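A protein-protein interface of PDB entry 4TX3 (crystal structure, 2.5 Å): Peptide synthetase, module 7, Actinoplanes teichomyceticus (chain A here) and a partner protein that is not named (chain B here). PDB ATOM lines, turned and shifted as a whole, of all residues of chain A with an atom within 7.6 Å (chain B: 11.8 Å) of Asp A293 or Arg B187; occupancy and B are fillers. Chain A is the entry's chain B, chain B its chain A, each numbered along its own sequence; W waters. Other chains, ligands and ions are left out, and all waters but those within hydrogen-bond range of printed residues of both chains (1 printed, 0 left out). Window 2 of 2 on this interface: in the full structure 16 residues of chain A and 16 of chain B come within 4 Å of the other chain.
Of the 10 printed residues of chain A, 4 touch a printed residue of chain B. Hydrophobic or aromatic side chains of chain A within 4 Å of the printed part of chain B: Ile A295. Of the 22 printed residues of chain B, 6 touch a printed residue of chain A. Among the printed residues, 7 pairs touch across the chains. Among the printed residues, Asp or Glu carboxylates within 4 Å of a Lys or Arg side-chain nitrogen of the other chain: Glu A292 with Arg B187, Glu A292 with Lys B188, Asp A293 with Arg B187 and Asp A296 with Arg B198.
N of Lys B188 sits at hydrogen-bond distance from OG of Ser B185. The side-chain carboxylate of Glu B194 lies within salt-bridge range of the guanidinium group of Arg B198, at 2.9 Å. The backbone NH (N) of Asp A293 lies within hydrogen-bond range of the side-chain carboxylate (OD1) of Asp A291 (3.1 Å).
Glu A292 touches just these residues of chain B: Arg B187 (2.7 Å) and Lys B188 (3.6 Å). Of the printed residues of chain B, Asp A293 touches Arg B187. Leu A294 touches none of the printed residues of chain B. Ile A295 touches just these residues of chain B: Ala B191 (3.1 Å), Glu B194 (3.6 Å) and Ala B195 (3.8 Å). Of the printed residues of chain B, Asp A296 touches Arg B198 (3.5 Å). Arg A306 touches none of the printed residues of chain B. Asp B181 touches none of the printed residues of chain A. Arg B187 touches two residues of chain A. Printed residues of chain A within 4 Å of Lys B188: Glu A292 (3.6 Å). Printed residues of chain A within 4 Å of Ala B191: Ile A295. Printed residues of chain A within 4 Å of Glu B194: Ile A295. Printed residues of chain A within 4 Å of Ala B195: Ile A295 (3.8 Å). The nearest residue of chain B that does not touch Asp A293 is Ala B191 (6.2 Å). The nearest printed residue of chain A that does not touch Ala B195 is Asp A296 (7.0 Å).
The guanidinium group of Arg B187 lies within salt-bridge range of the side-chain carboxylate of Glu A292, 2.7 Å away. The side-chain carboxylate (OD2) of Asp A293 is in salt-bridge range of the guanidinium group (NH2) of Arg B187, at 2.7 Å. NZ of Lys B188 lies within salt-bridge range of OE1 of Glu A292, at 3.6 Å. The side-chain carboxylate (OD1) of Asp A296 is in salt-bridge range of the guanidinium group (NH2) of Arg B198.
Among the printed residues, pairs that only touch across the chains: Ile A295 with Ala B191, Ile A295 with Glu B194 and Ile A295 with Ala B195.
Water W1 bridges the guanidinium group of Arg B198 and the backbone NH of Ile A295.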
ATOM      1  N   ARG A   5     -13.257  -5.950  -3.716  1.00  0.00           N
ATOM      2  CA  ARG A   5     -14.039  -7.177  -3.546  1.00  0.00           C
ATOM      3  C   ARG A   5     -14.911  -7.438  -4.763  1.00  0.00           C
ATOM      4  O   ARG A   5     -15.321  -6.500  -5.451  1.00  0.00           O
ATOM      5  CB  ARG A   5     -14.916  -7.097  -2.294  1.00  0.00           C
ATOM      6  CG  ARG A   5     -14.232  -6.425  -1.123  1.00  0.00           C
ATOM      7  CD  ARG A   5     -15.012  -6.564   0.180  1.00  0.00           C
ATOM      8  NE  ARG A   5     -16.159  -5.660   0.268  1.00  0.00           N
ATOM      9  CZ  ARG A   5     -16.913  -5.508   1.359  1.00  0.00           C
ATOM     10  NH1 ARG A   5     -16.645  -6.196   2.463  1.00  0.00           N
ATOM     11  NH2 ARG A   5     -17.934  -4.663   1.354  1.00  0.00           N
ATOM     12  N   ARG A 290     -22.464  -9.624  11.655  1.00  0.00           N
ATOM     13  CA  ARG A 290     -22.371  -9.358  10.232  1.00  0.00           C
ATOM     14  C   ARG A 290     -22.187  -7.863   9.955  1.00  0.00           C
ATOM     15  O   ARG A 290     -22.685  -7.016  10.688  1.00  0.00           O
ATOM     16  CB  ARG A 290     -23.620  -9.880   9.523  1.00  0.00           C
ATOM     17  CG  ARG A 290     -24.913  -9.262  10.009  1.00  0.00           C
ATOM     18  CD  ARG A 290     -26.139 -10.048   9.521  1.00  0.00           C
ATOM     19  NE  ARG A 290     -26.411 -11.219  10.355  1.00  0.00           N
ATOM     20  CZ  ARG A 290     -27.362 -12.117  10.110  1.00  0.00           C
ATOM     21  NH1 ARG A 290     -28.154 -11.994   9.048  1.00  0.00           N
ATOM     22  NH2 ARG A 290     -27.515 -13.150  10.925  1.00  0.00           N
ATOM     23  N   ASP A 291     -21.450  -7.557   8.900  1.00  0.00           N
ATOM     24  CA  ASP A 291     -21.271  -6.193   8.438  1.00  0.00           C
ATOM     25  C   ASP A 291     -22.622  -5.519   8.108  1.00  0.00           C
ATOM     26  O   ASP A 291     -23.305  -5.892   7.160  1.00  0.00           O
ATOM     27  CB  ASP A 291     -20.331  -6.226   7.235  1.00  0.00           C
ATOM     28  CG  ASP A 291     -20.069  -4.860   6.641  1.00  0.00           C
ATOM     29  OD1 ASP A 291     -20.526  -3.836   7.195  1.00  0.00           O
ATOM     30  OD2 ASP A 291     -19.382  -4.823   5.600  1.00  0.00           O
ATOM     31  N   GLU A 292     -23.004  -4.526   8.904  1.00  0.00           N
ATOM     32  CA  GLU A 292     -24.329  -3.909   8.792  1.00  0.00           C
ATOM     33  C   GLU A 292     -24.501  -3.143   7.475  1.00  0.00           C
ATOM     34  O   GLU A 292     -25.623  -2.888   7.035  1.00  0.00           O
ATOM     35  CB  GLU A 292     -24.584  -2.976   9.974  1.00  0.00           C
ATOM     36  CG  GLU A 292     -23.748  -1.694   9.960  1.00  0.00           C
ATOM     37  CD  GLU A 292     -24.033  -0.771  11.152  1.00  0.00           C
ATOM     38  OE1 GLU A 292     -24.638  -1.229  12.151  1.00  0.00           O
ATOM     39  OE2 GLU A 292     -23.661   0.423  11.081  1.00  0.00           O
ATOM     40  N   ASP A 293     -23.383  -2.788   6.848  1.00  0.00           N
ATOM     41  CA  ASP A 293     -23.398  -2.154   5.533  1.00  0.00           C
ATOM     42  C   ASP A 293     -23.914  -3.096   4.443  1.00  0.00           C
ATOM     43  O   ASP A 293     -24.506  -2.647   3.459  1.00  0.00           O
ATOM     44  CB  ASP A 293     -21.991  -1.657   5.159  1.00  0.00           C
ATOM     45  CG  ASP A 293     -21.570  -0.415   5.948  1.00  0.00           C
ATOM     46  OD1 ASP A 293     -22.448   0.248   6.554  1.00  0.00           O
ATOM     47  OD2 ASP A 293     -20.355  -0.100   5.958  1.00  0.00           O
ATOM     48  N   LEU A 294     -23.669  -4.395   4.606  1.00  0.00           N
ATOM     49  CA  LEU A 294     -24.165  -5.389   3.658  1.00  0.00           C
ATOM     50  C   LEU A 294     -25.657  -5.608   3.866  1.00  0.00           C
ATOM     51  O   LEU A 294     -26.057  -6.469   4.644  1.00  0.00           O
ATOM     52  CB  LEU A 294     -23.388  -6.704   3.800  1.00  0.00           C
ATOM     53  CG  LEU A 294     -21.873  -6.587   3.562  1.00  0.00           C
ATOM     54  CD1 LEU A 294     -21.222  -7.943   3.456  1.00  0.00           C
ATOM     55  CD2 LEU A 294     -21.575  -5.770   2.318  1.00  0.00           C
ATOM     56  N   ILE A 295     -26.473  -4.820   3.170  1.00  0.00           N
ATOM     57  CA  ILE A 295     -27.912  -4.788   3.438  1.00  0.00           C
ATOM     58  C   ILE A 295     -28.655  -6.101   3.141  1.00  0.00           C
ATOM     59  O   ILE A 295     -29.601  -6.461   3.858  1.00  0.00           O
ATOM     60  CB  ILE A 295     -28.583  -3.620   2.666  1.00  0.00           C
ATOM     61  CG1 ILE A 295     -28.391  -2.328   3.444  1.00  0.00           C
ATOM     62  CG2 ILE A 295     -30.067  -3.866   2.450  1.00  0.00           C
ATOM     63  CD1 ILE A 295     -29.390  -1.230   3.057  1.00  0.00           C
ATOM     64  N   ASP A 296     -28.214  -6.838   2.127  1.00  0.00           N
ATOM     65  CA  ASP A 296     -28.850  -8.099   1.782  1.00  0.00           C
ATOM     66  C   ASP A 296     -28.643  -9.219   2.793  1.00  0.00           C
ATOM     67  O   ASP A 296     -29.344 -10.230   2.728  1.00  0.00           O
ATOM     68  CB  ASP A 296     -28.366  -8.579   0.417  1.00  0.00           C
ATOM     69  CG  ASP A 296     -28.987  -7.802  -0.723  1.00  0.00           C
ATOM     70  OD1 ASP A 296     -29.958  -7.057  -0.472  1.00  0.00           O
ATOM     71  OD2 ASP A 296     -28.503  -7.935  -1.868  1.00  0.00           O
ATOM     72  N   LEU A 297     -27.684  -9.066   3.703  1.00  0.00           N
ATOM     73  CA  LEU A 297     -27.478 -10.067   4.751  1.00  0.00           C
ATOM     74  C   LEU A 297     -28.382  -9.885   5.978  1.00  0.00           C
ATOM     75  O   LEU A 297     -28.567 -10.837   6.749  1.00  0.00           O
ATOM     76  CB  LEU A 297     -26.023 -10.063   5.219  1.00  0.00           C
ATOM     77  CG  LEU A 297     -24.935 -10.172   4.156  1.00  0.00           C
ATOM     78  CD1 LEU A 297     -23.580 -10.119   4.836  1.00  0.00           C
ATOM     79  CD2 LEU A 297     -25.101 -11.448   3.351  1.00  0.00           C
ATOM     80  N   ARG A 306     -18.326 -12.932  13.086  1.00  0.00           N
ATOM     81  CA  ARG A 306     -16.900 -13.107  12.748  1.00  0.00           C
ATOM     82  C   ARG A 306     -15.956 -12.800  13.895  1.00  0.00           C
ATOM     83  O   ARG A 306     -15.952 -11.672  14.417  1.00  0.00           O
ATOM     84  CB  ARG A 306     -16.555 -12.203  11.583  1.00  0.00           C
ATOM     85  CG  ARG A 306     -17.376 -10.964  11.649  1.00  0.00           C
ATOM     86  CD  ARG A 306     -17.501 -10.282  10.339  1.00  0.00           C
ATOM     87  NE  ARG A 306     -18.208  -9.043  10.553  1.00  0.00           N
ATOM     88  CZ  ARG A 306     -17.836  -7.893  10.021  1.00  0.00           C
ATOM     89  NH1 ARG A 306     -16.749  -7.852   9.252  1.00  0.00           N
ATOM     90  NH2 ARG A 306     -18.529  -6.785  10.284  1.00  0.00           N
ATOM     91  N   LEU B 175     -38.719  -1.886   8.894  1.00  0.00           N
ATOM     92  CA  LEU B 175     -37.738  -1.072   8.189  1.00  0.00           C
ATOM     93  C   LEU B 175     -38.149   0.399   8.074  1.00  0.00           C
ATOM     94  O   LEU B 175     -37.308   1.276   8.233  1.00  0.00           O
ATOM     95  CB  LEU B 175     -37.480  -1.627   6.790  1.00  0.00           C
ATOM     96  CG  LEU B 175     -36.905  -3.033   6.694  1.00  0.00           C
ATOM     97  CD1 LEU B 175     -36.908  -3.477   5.245  1.00  0.00           C
ATOM     98  CD2 LEU B 175     -35.502  -3.094   7.281  1.00  0.00           C
ATOM     99  N   HIS B 177     -40.004   1.993  10.118  1.00  0.00           N
ATOM    100  CA  HIS B 177     -39.946   2.553  11.458  1.00  0.00           C
ATOM    101  C   HIS B 177     -38.502   2.738  11.906  1.00  0.00           C
ATOM    102  O   HIS B 177     -38.167   3.781  12.466  1.00  0.00           O
ATOM    103  CB  HIS B 177     -40.730   1.682  12.452  1.00  0.00           C
ATOM    104  CG  HIS B 177     -42.217   1.804  12.307  1.00  0.00           C
ATOM    105  ND1 HIS B 177     -43.100   0.916  12.879  1.00  0.00           N
ATOM    106  CD2 HIS B 177     -42.975   2.708  11.643  1.00  0.00           C
ATOM    107  CE1 HIS B 177     -44.339   1.270  12.581  1.00  0.00           C
ATOM    108  NE2 HIS B 177     -44.289   2.354  11.829  1.00  0.00           N
ATOM    109  N   ARG B 178     -37.645   1.747  11.647  1.00  0.00           N
ATOM    110  CA  ARG B 178     -36.216   1.879  11.956  1.00  0.00           C
ATOM    111  C   ARG B 178     -35.631   3.111  11.254  1.00  0.00           C
ATOM    112  O   ARG B 178     -34.844   3.858  11.841  1.00  0.00           O
ATOM    113  CB  ARG B 178     -35.443   0.622  11.548  1.00  0.00           C
ATOM    114  CG  ARG B 178     -35.672  -0.598  12.437  1.00  0.00           C
ATOM    115  CD  ARG B 178     -34.682  -1.727  12.132  1.00  0.00           C
ATOM    116  NE  ARG B 178     -33.290  -1.310  12.323  1.00  0.00           N
ATOM    117  CZ  ARG B 178     -32.601  -1.460  13.451  1.00  0.00           C
ATOM    118  NH1 ARG B 178     -33.162  -2.022  14.515  1.00  0.00           N
ATOM    119  NH2 ARG B 178     -31.344  -1.043  13.519  1.00  0.00           N
ATOM    120  N   HIS B 179     -36.056   3.326  10.009  1.00  0.00           N
ATOM    121  CA  HIS B 179     -35.586   4.436   9.180  1.00  0.00           C
ATOM    122  C   HIS B 179     -35.812   5.800   9.818  1.00  0.00           C
ATOM    123  O   HIS B 179     -35.080   6.745   9.542  1.00  0.00           O
ATOM    124  CB  HIS B 179     -36.272   4.399   7.815  1.00  0.00           C
ATOM    125  CG  HIS B 179     -36.012   5.611   6.976  1.00  0.00           C
ATOM    126  ND1 HIS B 179     -34.744   5.987   6.582  1.00  0.00           N
ATOM    127  CD2 HIS B 179     -36.858   6.538   6.462  1.00  0.00           C
ATOM    128  CE1 HIS B 179     -34.820   7.088   5.854  1.00  0.00           C
ATOM    129  NE2 HIS B 179     -36.091   7.447   5.771  1.00  0.00           N
ATOM    130  N   LEU B 180     -36.824   5.897  10.673  1.00  0.00           N
ATOM    131  CA  LEU B 180     -37.164   7.162  11.312  1.00  0.00           C
ATOM    132  C   LEU B 180     -36.854   7.182  12.819  1.00  0.00           C
ATOM    133  O   LEU B 180     -36.818   8.248  13.427  1.00  0.00           O
ATOM    134  CB  LEU B 180     -38.642   7.475  11.068  1.00  0.00           C
ATOM    135  CG  LEU B 180     -38.937   7.788   9.603  1.00  0.00           C
ATOM    136  CD1 LEU B 180     -40.418   7.678   9.314  1.00  0.00           C
ATOM    137  CD2 LEU B 180     -38.427   9.170   9.302  1.00  0.00           C
ATOM    138  N   ASP B 181     -36.629   6.012  13.411  1.00  0.00           N
ATOM    139  CA  ASP B 181     -36.313   5.901  14.838  1.00  0.00           C
ATOM    140  C   ASP B 181     -35.031   6.669  15.199  1.00  0.00           C
ATOM    141  O   ASP B 181     -33.917   6.166  15.028  1.00  0.00           O
ATOM    142  CB  ASP B 181     -36.188   4.420  15.232  1.00  0.00           C
ATOM    143  CG  ASP B 181     -35.801   4.225  16.688  1.00  0.00           C
ATOM    144  OD1 ASP B 181     -35.883   5.201  17.470  1.00  0.00           O
ATOM    145  OD2 ASP B 181     -35.423   3.087  17.056  1.00  0.00           O
ATOM    146  N   ALA B 182     -35.207   7.880  15.722  1.00  0.00           N
ATOM    147  CA  ALA B 182     -34.103   8.801  15.984  1.00  0.00           C
ATOM    148  C   ALA B 182     -33.071   8.252  16.976  1.00  0.00           C
ATOM    149  O   ALA B 182     -31.916   8.684  16.972  1.00  0.00           O
ATOM    150  CB  ALA B 182     -34.653  10.127  16.481  1.00  0.00           C
ATOM    151  N   SER B 183     -33.487   7.303  17.812  1.00  0.00           N
ATOM    152  CA  SER B 183     -32.600   6.705  18.806  1.00  0.00           C
ATOM    153  C   SER B 183     -31.471   5.901  18.165  1.00  0.00           C
ATOM    154  O   SER B 183     -30.381   5.778  18.728  1.00  0.00           O
ATOM    155  CB  SER B 183     -33.394   5.808  19.758  1.00  0.00           C
ATOM    156  OG  SER B 183     -33.636   4.529  19.192  1.00  0.00           O
ATOM    157  N   LEU B 184     -31.739   5.336  16.992  1.00  0.00           N
ATOM    158  CA  LEU B 184     -30.727   4.593  16.250  1.00  0.00           C
ATOM    159  C   LEU B 184     -29.798   5.581  15.573  1.00  0.00           C
ATOM    160  O   LEU B 184     -30.219   6.690  15.228  1.00  0.00           O
ATOM    161  CB  LEU B 184     -31.368   3.663  15.215  1.00  0.00           C
ATOM    162  CG  LEU B 184     -32.313   2.592  15.766  1.00  0.00           C
ATOM    163  CD1 LEU B 184     -32.979   1.803  14.642  1.00  0.00           C
ATOM    164  CD2 LEU B 184     -31.572   1.665  16.724  1.00  0.00           C
ATOM    165  N   SER B 185     -28.540   5.186  15.391  1.00  0.00           N
ATOM    166  CA  SER B 185     -27.561   6.029  14.714  1.00  0.00           C
ATOM    167  C   SER B 185     -28.017   6.352  13.293  1.00  0.00           C
ATOM    168  O   SER B 185     -28.729   5.562  12.666  1.00  0.00           O
ATOM    169  CB  SER B 185     -26.194   5.349  14.685  1.00  0.00           C
ATOM    170  OG  SER B 185     -26.233   4.180  13.890  1.00  0.00           O
ATOM    171  N   ALA B 186     -27.610   7.514  12.788  1.00  0.00           N
ATOM    172  CA  ALA B 186     -27.947   7.904  11.428  1.00  0.00           C
ATOM    173  C   ALA B 186     -27.421   6.878  10.419  1.00  0.00           C
ATOM    174  O   ALA B 186     -27.867   6.831   9.274  1.00  0.00           O
ATOM    175  CB  ALA B 186     -27.401   9.279  11.125  1.00  0.00           C
ATOM    176  N   ARG B 187     -26.477   6.048  10.851  1.00  0.00           N
ATOM    177  CA  ARG B 187     -25.979   4.970  10.010  1.00  0.00           C
ATOM    178  C   ARG B 187     -27.070   3.927   9.767  1.00  0.00           C
ATOM    179  O   ARG B 187     -27.535   3.761   8.635  1.00  0.00           O
ATOM    180  CB  ARG B 187     -24.748   4.318  10.643  1.00  0.00           C
ATOM    181  CG  ARG B 187     -23.937   3.483   9.668  1.00  0.00           C
ATOM    182  CD  ARG B 187     -22.464   3.869   9.717  1.00  0.00           C
ATOM    183  NE  ARG B 187     -21.656   3.021   8.847  1.00  0.00           N
ATOM    184  CZ  ARG B 187     -21.115   1.866   9.219  1.00  0.00           C
ATOM    185  NH1 ARG B 187     -21.283   1.413  10.454  1.00  0.00           N
ATOM    186  NH2 ARG B 187     -20.402   1.162   8.353  1.00  0.00           N
ATOM    187  N   LYS B 188     -27.464   3.233  10.834  1.00  0.00           N
ATOM    188  CA  LYS B 188     -28.563   2.269  10.811  1.00  0.00           C
ATOM    189  C   LYS B 188     -29.816   2.813  10.106  1.00  0.00           C
ATOM    190  O   LYS B 188     -30.484   2.097   9.358  1.00  0.00           O
ATOM    191  CB  LYS B 188     -28.926   1.849  12.241  1.00  0.00           C
ATOM    192  CG  LYS B 188     -27.787   1.202  13.010  1.00  0.00           C
ATOM    193  CD  LYS B 188     -28.140   1.022  14.485  1.00  0.00           C
ATOM    194  CE  LYS B 188     -27.043   0.255  15.229  1.00  0.00           C
ATOM    195  NZ  LYS B 188     -25.674   0.774  14.935  1.00  0.00           N
ATOM    196  N   ARG B 189     -30.123   4.082  10.345  1.00  0.00           N
ATOM    197  CA  ARG B 189     -31.329   4.679   9.797  1.00  0.00           C
ATOM    198  C   ARG B 189     -31.268   4.775   8.282  1.00  0.00           C
ATOM    199  O   ARG B 189     -32.246   4.460   7.589  1.00  0.00           O
ATOM    200  CB  ARG B 189     -31.570   6.053  10.426  1.00  0.00           C
ATOM    201  CG  ARG B 189     -32.044   5.938  11.876  1.00  0.00           C
ATOM    202  CD  ARG B 189     -32.043   7.268  12.619  1.00  0.00           C
ATOM    203  NE  ARG B 189     -32.805   8.293  11.916  1.00  0.00           N
ATOM    204  CZ  ARG B 189     -32.281   9.427  11.461  1.00  0.00           C
ATOM    205  NH1 ARG B 189     -30.989   9.689  11.651  1.00  0.00           N
ATOM    206  NH2 ARG B 189     -33.048  10.305  10.820  1.00  0.00           N
ATOM    207  N   ALA B 190     -30.122   5.189   7.758  1.00  0.00           N
ATOM    208  CA  ALA B 190     -29.962   5.253   6.313  1.00  0.00           C
ATOM    209  C   ALA B 190     -30.000   3.834   5.738  1.00  0.00           C
ATOM    210  O   ALA B 190     -30.578   3.601   4.671  1.00  0.00           O
ATOM    211  CB  ALA B 190     -28.672   5.959   5.945  1.00  0.00           C
ATOM    212  N   ALA B 191     -29.393   2.892   6.460  1.00  0.00           N
ATOM    213  CA  ALA B 191     -29.461   1.485   6.094  1.00  0.00           C
ATOM    214  C   ALA B 191     -30.916   1.018   5.938  1.00  0.00           C
ATOM    215  O   ALA B 191     -31.293   0.474   4.890  1.00  0.00           O
ATOM    216  CB  ALA B 191     -28.747   0.642   7.124  1.00  0.00           C
ATOM    217  N   ALA B 192     -31.725   1.242   6.976  1.00  0.00           N
ATOM    218  CA  ALA B 192     -33.111   0.776   6.985  1.00  0.00           C
ATOM    219  C   ALA B 192     -33.916   1.433   5.872  1.00  0.00           C
ATOM    220  O   ALA B 192     -34.749   0.783   5.230  1.00  0.00           O
ATOM    221  CB  ALA B 192     -33.766   1.040   8.334  1.00  0.00           C
ATOM    222  N   GLY B 193     -33.664   2.718   5.645  1.00  0.00           N
ATOM    223  CA  GLY B 193     -34.317   3.437   4.562  1.00  0.00           C
ATOM    224  C   GLY B 193     -34.018   2.837   3.195  1.00  0.00           C
ATOM    225  O   GLY B 193     -34.925   2.656   2.375  1.00  0.00           O
ATOM    226  N   GLU B 194     -32.745   2.520   2.958  1.00  0.00           N
ATOM    227  CA  GLU B 194     -32.314   1.933   1.698  1.00  0.00           C
ATOM    228  C   GLU B 194     -32.991   0.587   1.467  1.00  0.00           C
ATOM    229  O   GLU B 194     -33.523   0.317   0.380  1.00  0.00           O
ATOM    230  CB  GLU B 194     -30.792   1.768   1.679  1.00  0.00           C
ATOM    231  CG  GLU B 194     -30.099   2.534   0.560  1.00  0.00           C
ATOM    232  CD  GLU B 194     -30.420   1.992  -0.829  1.00  0.00           C
ATOM    233  OE1 GLU B 194     -30.044   0.832  -1.128  1.00  0.00           O
ATOM    234  OE2 GLU B 194     -31.045   2.737  -1.624  1.00  0.00           O
ATOM    235  N   ALA B 195     -32.979  -0.246   2.504  1.00  0.00           N
ATOM    236  CA  ALA B 195     -33.566  -1.570   2.416  1.00  0.00           C
ATOM    237  C   ALA B 195     -35.074  -1.521   2.078  1.00  0.00           C
ATOM    238  O   ALA B 195     -35.546  -2.334   1.271  1.00  0.00           O
ATOM    239  CB  ALA B 195     -33.324  -2.332   3.702  1.00  0.00           C
ATOM    240  N   PHE B 196     -35.832  -0.575   2.638  1.00  0.00           N
ATOM    241  CA  PHE B 196     -37.266  -0.620   2.340  1.00  0.00           C
ATOM    242  C   PHE B 196     -37.530   0.042   0.986  1.00  0.00           C
ATOM    243  O   PHE B 196     -38.517  -0.271   0.313  1.00  0.00           O
ATOM    244  CB  PHE B 196     -38.132  -0.043   3.500  1.00  0.00           C
ATOM    245  CG  PHE B 196     -38.477   1.433   3.419  1.00  0.00           C
ATOM    246  CD1 PHE B 196     -39.497   1.887   2.586  1.00  0.00           C
ATOM    247  CD2 PHE B 196     -37.910   2.334   4.312  1.00  0.00           C
ATOM    248  CE1 PHE B 196     -39.856   3.232   2.556  1.00  0.00           C
ATOM    249  CE2 PHE B 196     -38.266   3.683   4.295  1.00  0.00           C
ATOM    250  CZ  PHE B 196     -39.241   4.130   3.415  1.00  0.00           C
ATOM    251  N   ARG B 198     -35.270  -0.521  -1.491  1.00  0.00           N
ATOM    252  CA  ARG B 198     -34.901  -1.658  -2.341  1.00  0.00           C
ATOM    253  C   ARG B 198     -36.104  -2.581  -2.509  1.00  0.00           C
ATOM    254  O   ARG B 198     -36.369  -3.120  -3.594  1.00  0.00           O
ATOM    255  CB  ARG B 198     -33.716  -2.446  -1.749  1.00  0.00           C
ATOM    256  CG  ARG B 198     -32.381  -1.686  -1.701  1.00  0.00           C
ATOM    257  CD  ARG B 198     -31.402  -2.133  -2.776  1.00  0.00           C
ATOM    258  NE  ARG B 198     -30.496  -3.192  -2.323  1.00  0.00           N
ATOM    259  CZ  ARG B 198     -29.277  -2.981  -1.824  1.00  0.00           C
ATOM    260  NH1 ARG B 198     -28.803  -1.743  -1.703  1.00  0.00           N
ATOM    261  NH2 ARG B 198     -28.528  -4.011  -1.443  1.00  0.00           N
HETATM  262  O   HOH W   1     -26.153  -3.684   0.303  1.00  0.00           O
